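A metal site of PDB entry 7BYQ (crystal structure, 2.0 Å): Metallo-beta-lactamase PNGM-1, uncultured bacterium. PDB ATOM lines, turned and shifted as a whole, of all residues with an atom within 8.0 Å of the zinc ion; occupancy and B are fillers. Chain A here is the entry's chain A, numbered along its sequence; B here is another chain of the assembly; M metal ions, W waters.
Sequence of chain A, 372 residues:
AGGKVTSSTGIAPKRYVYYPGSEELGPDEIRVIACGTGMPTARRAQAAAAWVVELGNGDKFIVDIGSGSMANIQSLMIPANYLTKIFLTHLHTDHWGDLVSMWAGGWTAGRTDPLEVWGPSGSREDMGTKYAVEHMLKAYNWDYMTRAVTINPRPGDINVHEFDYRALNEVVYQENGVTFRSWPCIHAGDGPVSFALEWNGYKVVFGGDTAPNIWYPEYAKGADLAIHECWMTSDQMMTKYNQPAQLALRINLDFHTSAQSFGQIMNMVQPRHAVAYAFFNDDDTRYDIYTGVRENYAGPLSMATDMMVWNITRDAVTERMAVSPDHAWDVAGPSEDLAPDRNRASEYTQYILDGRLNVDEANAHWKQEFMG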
ATOM      1  N   MET A  39      15.294 -21.226  14.998  1.00  0.00           N
ATOM      2  CA  MET A  39      15.732 -22.565  14.497  1.00  0.00           C
ATOM      3  C   MET A  39      16.048 -23.477  15.682  1.00  0.00           C
ATOM      4  O   MET A  39      15.198 -23.631  16.553  1.00  0.00           O
ATOM      5  CB  MET A  39      16.927 -22.349  13.548  1.00  0.00           C
ATOM      6  CG  MET A  39      16.948 -23.267  12.324  1.00  0.00           C
ATOM      7  SD  MET A  39      16.366 -22.448  10.823  1.00  0.00           S
ATOM      8  CE  MET A  39      16.655 -23.709   9.584  1.00  0.00           C
ATOM      9  N   ALA A  49      10.802 -21.249  19.242  1.00  0.00           N
ATOM     10  CA  ALA A  49       9.334 -21.440  19.180  1.00  0.00           C
ATOM     11  C   ALA A  49       8.681 -21.076  20.501  1.00  0.00           C
ATOM     12  O   ALA A  49       9.027 -21.710  21.530  1.00  0.00           O
ATOM     13  CB  ALA A  49       9.025 -22.871  18.811  1.00  0.00           C
ATOM     14  N   ASP A  64       4.001 -23.616  23.399  1.00  0.00           N
ATOM     15  CA  ASP A  64       5.487 -23.705  23.336  1.00  0.00           C
ATOM     16  C   ASP A  64       6.114 -22.488  24.031  1.00  0.00           C
ATOM     17  O   ASP A  64       5.568 -21.366  23.881  1.00  0.00           O
ATOM     18  CB  ASP A  64       6.011 -23.898  21.906  1.00  0.00           C
ATOM     19  CG  ASP A  64       5.766 -25.274  21.308  1.00  0.00           C
ATOM     20  OD1 ASP A  64       5.374 -26.191  22.061  1.00  0.00           O
ATOM     21  OD2 ASP A  64       5.936 -25.412  20.074  1.00  0.00           O
ATOM     22  N   THR A  89       4.301 -28.692  22.205  1.00  0.00           N
ATOM     23  CA  THR A  89       4.169 -29.500  20.963  1.00  0.00           C
ATOM     24  C   THR A  89       5.210 -30.620  20.966  1.00  0.00           C
ATOM     25  O   THR A  89       5.125 -31.480  20.103  1.00  0.00           O
ATOM     26  CB  THR A  89       4.329 -28.630  19.713  1.00  0.00           C
ATOM     27  OG1 THR A  89       5.664 -28.139  19.721  1.00  0.00           O
ATOM     28  CG2 THR A  89       3.330 -27.496  19.655  1.00  0.00           C
ATOM     29  N   HIS A  90       6.184 -30.560  21.866  1.00  0.00           N
ATOM     30  CA  HIS A  90       7.181 -31.634  22.119  1.00  0.00           C
ATOM     31  C   HIS A  90       8.247 -31.124  23.092  1.00  0.00           C
ATOM     32  O   HIS A  90       8.185 -29.935  23.460  1.00  0.00           O
ATOM     33  CB  HIS A  90       7.757 -32.185  20.820  1.00  0.00           C
ATOM     34  CG  HIS A  90       8.430 -31.200  19.931  1.00  0.00           C
ATOM     35  ND1 HIS A  90       7.837 -30.023  19.516  1.00  0.00           N
ATOM     36  CD2 HIS A  90       9.637 -31.249  19.322  1.00  0.00           C
ATOM     37  CE1 HIS A  90       8.663 -29.377  18.713  1.00  0.00           C
ATOM     38  NE2 HIS A  90       9.777 -30.112  18.569  1.00  0.00           N
ATOM     39  N   LEU A  91       9.178 -31.999  23.486  1.00  0.00           N
ATOM     40  CA  LEU A  91      10.107 -31.803  24.625  1.00  0.00           C
ATOM     41  C   LEU A  91      11.517 -31.507  24.110  1.00  0.00           C
ATOM     42  O   LEU A  91      12.489 -31.693  24.868  1.00  0.00           O
ATOM     43  CB  LEU A  91      10.038 -33.023  25.543  1.00  0.00           C
ATOM     44  CG  LEU A  91       8.658 -33.312  26.136  1.00  0.00           C
ATOM     45  CD1 LEU A  91       8.637 -34.643  26.885  1.00  0.00           C
ATOM     46  CD2 LEU A  91       8.206 -32.185  27.057  1.00  0.00           C
ATOM     47  N   HIS A  92      11.631 -31.009  22.875  1.00  0.00           N
ATOM     48  CA  HIS A  92      12.840 -30.323  22.376  1.00  0.00           C
ATOM     49  C   HIS A  92      13.051 -29.071  23.230  1.00  0.00           C
ATOM     50  O   HIS A  92      12.040 -28.372  23.472  1.00  0.00           O
ATOM     51  CB  HIS A  92      12.737 -30.001  20.883  1.00  0.00           C
ATOM     52  CG  HIS A  92      13.264 -31.085  20.008  1.00  0.00           C
ATOM     53  ND1 HIS A  92      12.814 -31.286  18.720  1.00  0.00           N
ATOM     54  CD2 HIS A  92      14.191 -32.045  20.243  1.00  0.00           C
ATOM     55  CE1 HIS A  92      13.462 -32.305  18.183  1.00  0.00           C
ATOM     56  NE2 HIS A  92      14.285 -32.808  19.113  1.00  0.00           N
ATOM     57  N   THR A  93      14.293 -28.812  23.651  1.00  0.00           N
ATOM     58  CA  THR A  93      14.695 -27.646  24.487  1.00  0.00           C
ATOM     59  C   THR A  93      14.133 -26.384  23.831  1.00  0.00           C
ATOM     60  O   THR A  93      13.622 -25.525  24.549  1.00  0.00           O
ATOM     61  CB  THR A  93      16.217 -27.544  24.644  1.00  0.00           C
ATOM     62  OG1 THR A  93      16.817 -27.413  23.354  1.00  0.00           O
ATOM     63  CG2 THR A  93      16.838 -28.730  25.349  1.00  0.00           C
ATOM     64  N   ASP A  94      14.163 -26.355  22.494  1.00  0.00           N
ATOM     65  CA  ASP A  94      13.766 -25.207  21.637  1.00  0.00           C
ATOM     66  C   ASP A  94      12.258 -24.998  21.683  1.00  0.00           C
ATOM     67  O   ASP A  94      11.786 -24.207  20.893  1.00  0.00           O
ATOM     68  CB  ASP A  94      14.190 -25.481  20.186  1.00  0.00           C
ATOM     69  CG  ASP A  94      15.673 -25.341  19.989  1.00  0.00           C
ATOM     70  OD1 ASP A  94      16.253 -24.376  20.561  1.00  0.00           O
ATOM     71  OD2 ASP A  94      16.236 -26.176  19.242  1.00  0.00           O
ATOM     72  N   HIS A  95      11.528 -25.705  22.554  1.00  0.00           N
ATOM     73  CA  HIS A  95      10.039 -25.721  22.578  1.00  0.00           C
ATOM     74  C   HIS A  95       9.495 -25.638  24.014  1.00  0.00           C
ATOM     75  O   HIS A  95       8.306 -25.336  24.128  1.00  0.00           O
ATOM     76  CB  HIS A  95       9.518 -26.937  21.785  1.00  0.00           C
ATOM     77  CG  HIS A  95       9.465 -26.724  20.305  1.00  0.00           C
ATOM     78  ND1 HIS A  95       8.316 -26.300  19.659  1.00  0.00           N
ATOM     79  CD2 HIS A  95      10.406 -26.857  19.352  1.00  0.00           C
ATOM     80  CE1 HIS A  95       8.554 -26.168  18.372  1.00  0.00           C
ATOM     81  NE2 HIS A  95       9.822 -26.521  18.155  1.00  0.00           N
ATOM     82  N   HIS A 187       8.589 -36.511  13.835  1.00  0.00           N
ATOM     83  CA  HIS A 187       9.671 -35.588  14.297  1.00  0.00           C
ATOM     84  C   HIS A 187      10.559 -36.166  15.402  1.00  0.00           C
ATOM     85  O   HIS A 187      10.092 -36.266  16.537  1.00  0.00           O
ATOM     86  CB  HIS A 187       9.044 -34.286  14.794  1.00  0.00           C
ATOM     87  CG  HIS A 187      10.091 -33.267  15.118  1.00  0.00           C
ATOM     88  ND1 HIS A 187      10.841 -32.661  14.142  1.00  0.00           N
ATOM     89  CD2 HIS A 187      10.549 -32.827  16.298  1.00  0.00           C
ATOM     90  CE1 HIS A 187      11.698 -31.844  14.711  1.00  0.00           C
ATOM     91  NE2 HIS A 187      11.501 -31.885  16.037  1.00  0.00           N
ATOM     92  N   ALA A 188      11.828 -36.426  15.069  1.00  0.00           N
ATOM     93  CA  ALA A 188      12.927 -36.827  15.988  1.00  0.00           C
ATOM     94  C   ALA A 188      12.749 -38.300  16.408  1.00  0.00           C
ATOM     95  O   ALA A 188      13.764 -38.982  16.443  1.00  0.00           O
ATOM     96  CB  ALA A 188      12.995 -35.928  17.196  1.00  0.00           C
ATOM     97  N   PRO A 192       6.070 -35.957  19.475  1.00  0.00           N
ATOM     98  CA  PRO A 192       5.595 -34.609  19.106  1.00  0.00           C
ATOM     99  C   PRO A 192       4.197 -34.510  18.479  1.00  0.00           C
ATOM    100  O   PRO A 192       3.800 -35.403  17.728  1.00  0.00           O
ATOM    101  CB  PRO A 192       6.683 -34.141  18.122  1.00  0.00           C
ATOM    102  CG  PRO A 192       7.889 -34.943  18.518  1.00  0.00           C
ATOM    103  CD  PRO A 192       7.319 -36.323  18.780  1.00  0.00           C
ATOM    104  N   GLY A 208       3.752 -26.846  15.259  1.00  0.00           N
ATOM    105  CA  GLY A 208       4.933 -27.330  15.996  1.00  0.00           C
ATOM    106  C   GLY A 208       6.061 -27.680  15.044  1.00  0.00           C
ATOM    107  O   GLY A 208       6.450 -26.792  14.235  1.00  0.00           O
ATOM    108  N   ASP A 209       6.563 -28.931  15.125  1.00  0.00           N
ATOM    109  CA  ASP A 209       7.551 -29.521  14.184  1.00  0.00           C
ATOM    110  C   ASP A 209       7.023 -30.874  13.711  1.00  0.00           C
ATOM    111  O   ASP A 209       6.278 -31.526  14.474  1.00  0.00           O
ATOM    112  CB  ASP A 209       8.946 -29.693  14.808  1.00  0.00           C
ATOM    113  CG  ASP A 209       9.524 -28.394  15.329  1.00  0.00           C
ATOM    114  OD1 ASP A 209       8.732 -27.537  15.710  1.00  0.00           O
ATOM    115  OD2 ASP A 209      10.765 -28.256  15.352  1.00  0.00           O
ATOM    116  N   THR A 210       7.394 -31.252  12.493  1.00  0.00           N
ATOM    117  CA  THR A 210       6.826 -32.390  11.721  1.00  0.00           C
ATOM    118  C   THR A 210       7.322 -32.339  10.275  1.00  0.00           C
ATOM    119  O   THR A 210       7.279 -31.244   9.689  1.00  0.00           O
ATOM    120  CB  THR A 210       5.293 -32.369  11.714  1.00  0.00           C
ATOM    121  OG1 THR A 210       4.846 -33.570  11.092  1.00  0.00           O
ATOM    122  CG2 THR A 210       4.703 -31.163  11.001  1.00  0.00           C
ATOM    123  N   GLU A 229       5.749 -25.449  10.517  1.00  0.00           N
ATOM    124  CA  GLU A 229       7.173 -25.522  10.153  1.00  0.00           C
ATOM    125  C   GLU A 229       7.324 -25.131   8.683  1.00  0.00           C
ATOM    126  O   GLU A 229       6.481 -25.550   7.861  1.00  0.00           O
ATOM    127  CB  GLU A 229       7.682 -26.939  10.398  1.00  0.00           C
ATOM    128  CG  GLU A 229       9.033 -27.214   9.765  1.00  0.00           C
ATOM    129  CD  GLU A 229       9.742 -28.395  10.388  1.00  0.00           C
ATOM    130  OE1 GLU A 229       9.581 -28.596  11.604  1.00  0.00           O
ATOM    131  OE2 GLU A 229      10.437 -29.106   9.655  1.00  0.00           O
ATOM    132  N   TRP A 231      10.969 -24.916   6.497  1.00  0.00           N
ATOM    133  CA  TRP A 231      12.441 -25.054   6.665  1.00  0.00           C
ATOM    134  C   TRP A 231      13.137 -24.102   5.689  1.00  0.00           C
ATOM    135  O   TRP A 231      12.439 -23.530   4.821  1.00  0.00           O
ATOM    136  CB  TRP A 231      12.894 -26.515   6.504  1.00  0.00           C
ATOM    137  CG  TRP A 231      14.019 -26.884   7.412  1.00  0.00           C
ATOM    138  CD1 TRP A 231      15.292 -27.241   7.058  1.00  0.00           C
ATOM    139  CD2 TRP A 231      13.990 -26.882   8.851  1.00  0.00           C
ATOM    140  NE1 TRP A 231      16.051 -27.470   8.179  1.00  0.00           N
ATOM    141  CE2 TRP A 231      15.276 -27.268   9.292  1.00  0.00           C
ATOM    142  CE3 TRP A 231      13.010 -26.600   9.807  1.00  0.00           C
ATOM    143  CZ2 TRP A 231      15.603 -27.359  10.641  1.00  0.00           C
ATOM    144  CZ3 TRP A 231      13.323 -26.715  11.147  1.00  0.00           C
ATOM    145  CH2 TRP A 231      14.597 -27.091  11.554  1.00  0.00           C
ATOM    146  N   PHE A 255      13.387 -34.984   6.983  1.00  0.00           N
ATOM    147  CA  PHE A 255      13.549 -34.623   8.423  1.00  0.00           C
ATOM    148  C   PHE A 255      12.728 -33.377   8.766  1.00  0.00           C
ATOM    149  O   PHE A 255      12.355 -33.243   9.955  1.00  0.00           O
ATOM    150  CB  PHE A 255      15.027 -34.418   8.739  1.00  0.00           C
ATOM    151  CG  PHE A 255      15.905 -35.588   8.379  1.00  0.00           C
ATOM    152  CD1 PHE A 255      15.482 -36.887   8.609  1.00  0.00           C
ATOM    153  CD2 PHE A 255      17.155 -35.388   7.815  1.00  0.00           C
ATOM    154  CE1 PHE A 255      16.286 -37.965   8.275  1.00  0.00           C
ATOM    155  CE2 PHE A 255      17.956 -36.474   7.485  1.00  0.00           C
ATOM    156  CZ  PHE A 255      17.519 -37.756   7.714  1.00  0.00           C
ATOM    157  N   HIS A 256      12.482 -32.496   7.795  1.00  0.00           N
ATOM    158  CA  HIS A 256      11.791 -31.186   7.994  1.00  0.00           C
ATOM    159  C   HIS A 256      10.989 -30.833   6.738  1.00  0.00           C
ATOM    160  O   HIS A 256      11.402 -31.215   5.631  1.00  0.00           O
ATOM    161  CB  HIS A 256      12.806 -30.087   8.355  1.00  0.00           C
ATOM    162  CG  HIS A 256      13.514 -30.323   9.647  1.00  0.00           C
ATOM    163  ND1 HIS A 256      12.844 -30.426  10.851  1.00  0.00           N
ATOM    164  CD2 HIS A 256      14.819 -30.476   9.932  1.00  0.00           C
ATOM    165  CE1 HIS A 256      13.705 -30.643  11.824  1.00  0.00           C
ATOM    166  NE2 HIS A 256      14.931 -30.660  11.286  1.00  0.00           N
ATOM    167  N   TYR A 277       6.947 -20.568  10.097  1.00  0.00           N
ATOM    168  CA  TYR A 277       7.921 -20.280  11.171  1.00  0.00           C
ATOM    169  C   TYR A 277       8.944 -21.411  11.229  1.00  0.00           C
ATOM    170  O   TYR A 277       8.902 -22.323  10.370  1.00  0.00           O
ATOM    171  CB  TYR A 277       7.187 -20.036  12.502  1.00  0.00           C
ATOM    172  CG  TYR A 277       7.038 -21.261  13.373  1.00  0.00           C
ATOM    173  CD1 TYR A 277       6.025 -22.185  13.159  1.00  0.00           C
ATOM    174  CD2 TYR A 277       7.908 -21.507  14.412  1.00  0.00           C
ATOM    175  CE1 TYR A 277       5.879 -23.308  13.955  1.00  0.00           C
ATOM    176  CE2 TYR A 277       7.790 -22.623  15.217  1.00  0.00           C
ATOM    177  CZ  TYR A 277       6.775 -23.526  14.995  1.00  0.00           C
ATOM    178  OH  TYR A 277       6.659 -24.635  15.796  1.00  0.00           O
ATOM    179  N   TRP B 142      13.627 -37.226  26.397  1.00  0.00           N
ATOM    180  CA  TRP B 142      13.021 -37.311  25.055  1.00  0.00           C
ATOM    181  C   TRP B 142      13.964 -36.686  24.032  1.00  0.00           C
ATOM    182  O   TRP B 142      14.007 -37.229  22.892  1.00  0.00           O
ATOM    183  CB  TRP B 142      11.629 -36.666  24.988  1.00  0.00           C
ATOM    184  CG  TRP B 142      11.053 -36.861  23.620  1.00  0.00           C
ATOM    185  CD1 TRP B 142      10.377 -37.946  23.155  1.00  0.00           C
ATOM    186  CD2 TRP B 142      11.223 -35.975  22.497  1.00  0.00           C
ATOM    187  NE1 TRP B 142      10.060 -37.780  21.842  1.00  0.00           N
ATOM    188  CE2 TRP B 142      10.585 -36.584  21.407  1.00  0.00           C
ATOM    189  CE3 TRP B 142      11.841 -34.736  22.318  1.00  0.00           C
ATOM    190  CZ2 TRP B 142      10.522 -35.978  20.154  1.00  0.00           C
ATOM    191  CZ3 TRP B 142      11.769 -34.131  21.079  1.00  0.00           C
ATOM    192  CH2 TRP B 142      11.131 -34.750  20.016  1.00  0.00           C
ATOM    193  N   ASP B 143      14.647 -35.606  24.427  1.00  0.00           N
ATOM    194  CA  ASP B 143      15.578 -34.803  23.589  1.00  0.00           C
ATOM    195  C   ASP B 143      16.824 -35.639  23.331  1.00  0.00           C
ATOM    196  O   ASP B 143      17.181 -35.875  22.143  1.00  0.00           O
ATOM    197  CB  ASP B 143      15.921 -33.479  24.295  1.00  0.00           C
ATOM    198  CG  ASP B 143      16.800 -32.529  23.511  1.00  0.00           C
ATOM    199  OD1 ASP B 143      16.258 -31.799  22.691  1.00  0.00           O
ATOM    200  OD2 ASP B 143      18.028 -32.541  23.736  1.00  0.00           O
HETATM  201 ZN    ZN M   1      11.123 -30.015  17.002  1.00  0.00          ZN
HETATM  202  O   HOH W   1      13.284 -28.986  17.906  1.00  0.00           O
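NE2 of His 90 lies close to ND1 of His 92 (3.3 Å).
A ring nitrogen (ND1) of His 90 sits at hydrogen-bond distance from the side-chain hydroxyl of Thr 89, 2.9 Å away.
ND1 of His 92 lies close to NE2 of His 187, 3.0 Å away.
OD1 of Asp 209 is in hydrogen-bond range of NE2 of His 95 (2.9 Å).
ND1 of His 95 is in hydrogen-bond range of OG1 of Thr 89, at 3.2 Å.
The side-chain carboxylate (OD2) of Asp 64 sits at hydrogen-bond distance from a ring nitrogen (ND1) of His 95 (2.6 Å).
The zinc ion is bound by NE2 of His 90 (2.1 Å), NE2 of His 187 (2.1 Å), OD2 of Asp 209 (2.4 Å) and water W1 (2.6 Å).
The zinc ion has four donor atoms within binding distance.
Slightly farther from the zinc ion lies ND1 of His 92 (2.7 Å).
Merely in contact with the zinc ion: His 95 (3.9 Å).
Of the 23 residues printed, 5 come within 4 Å of the zinc ion.
Along chain A the residues within 4 Å of the zinc ion span positions 90 to 209.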
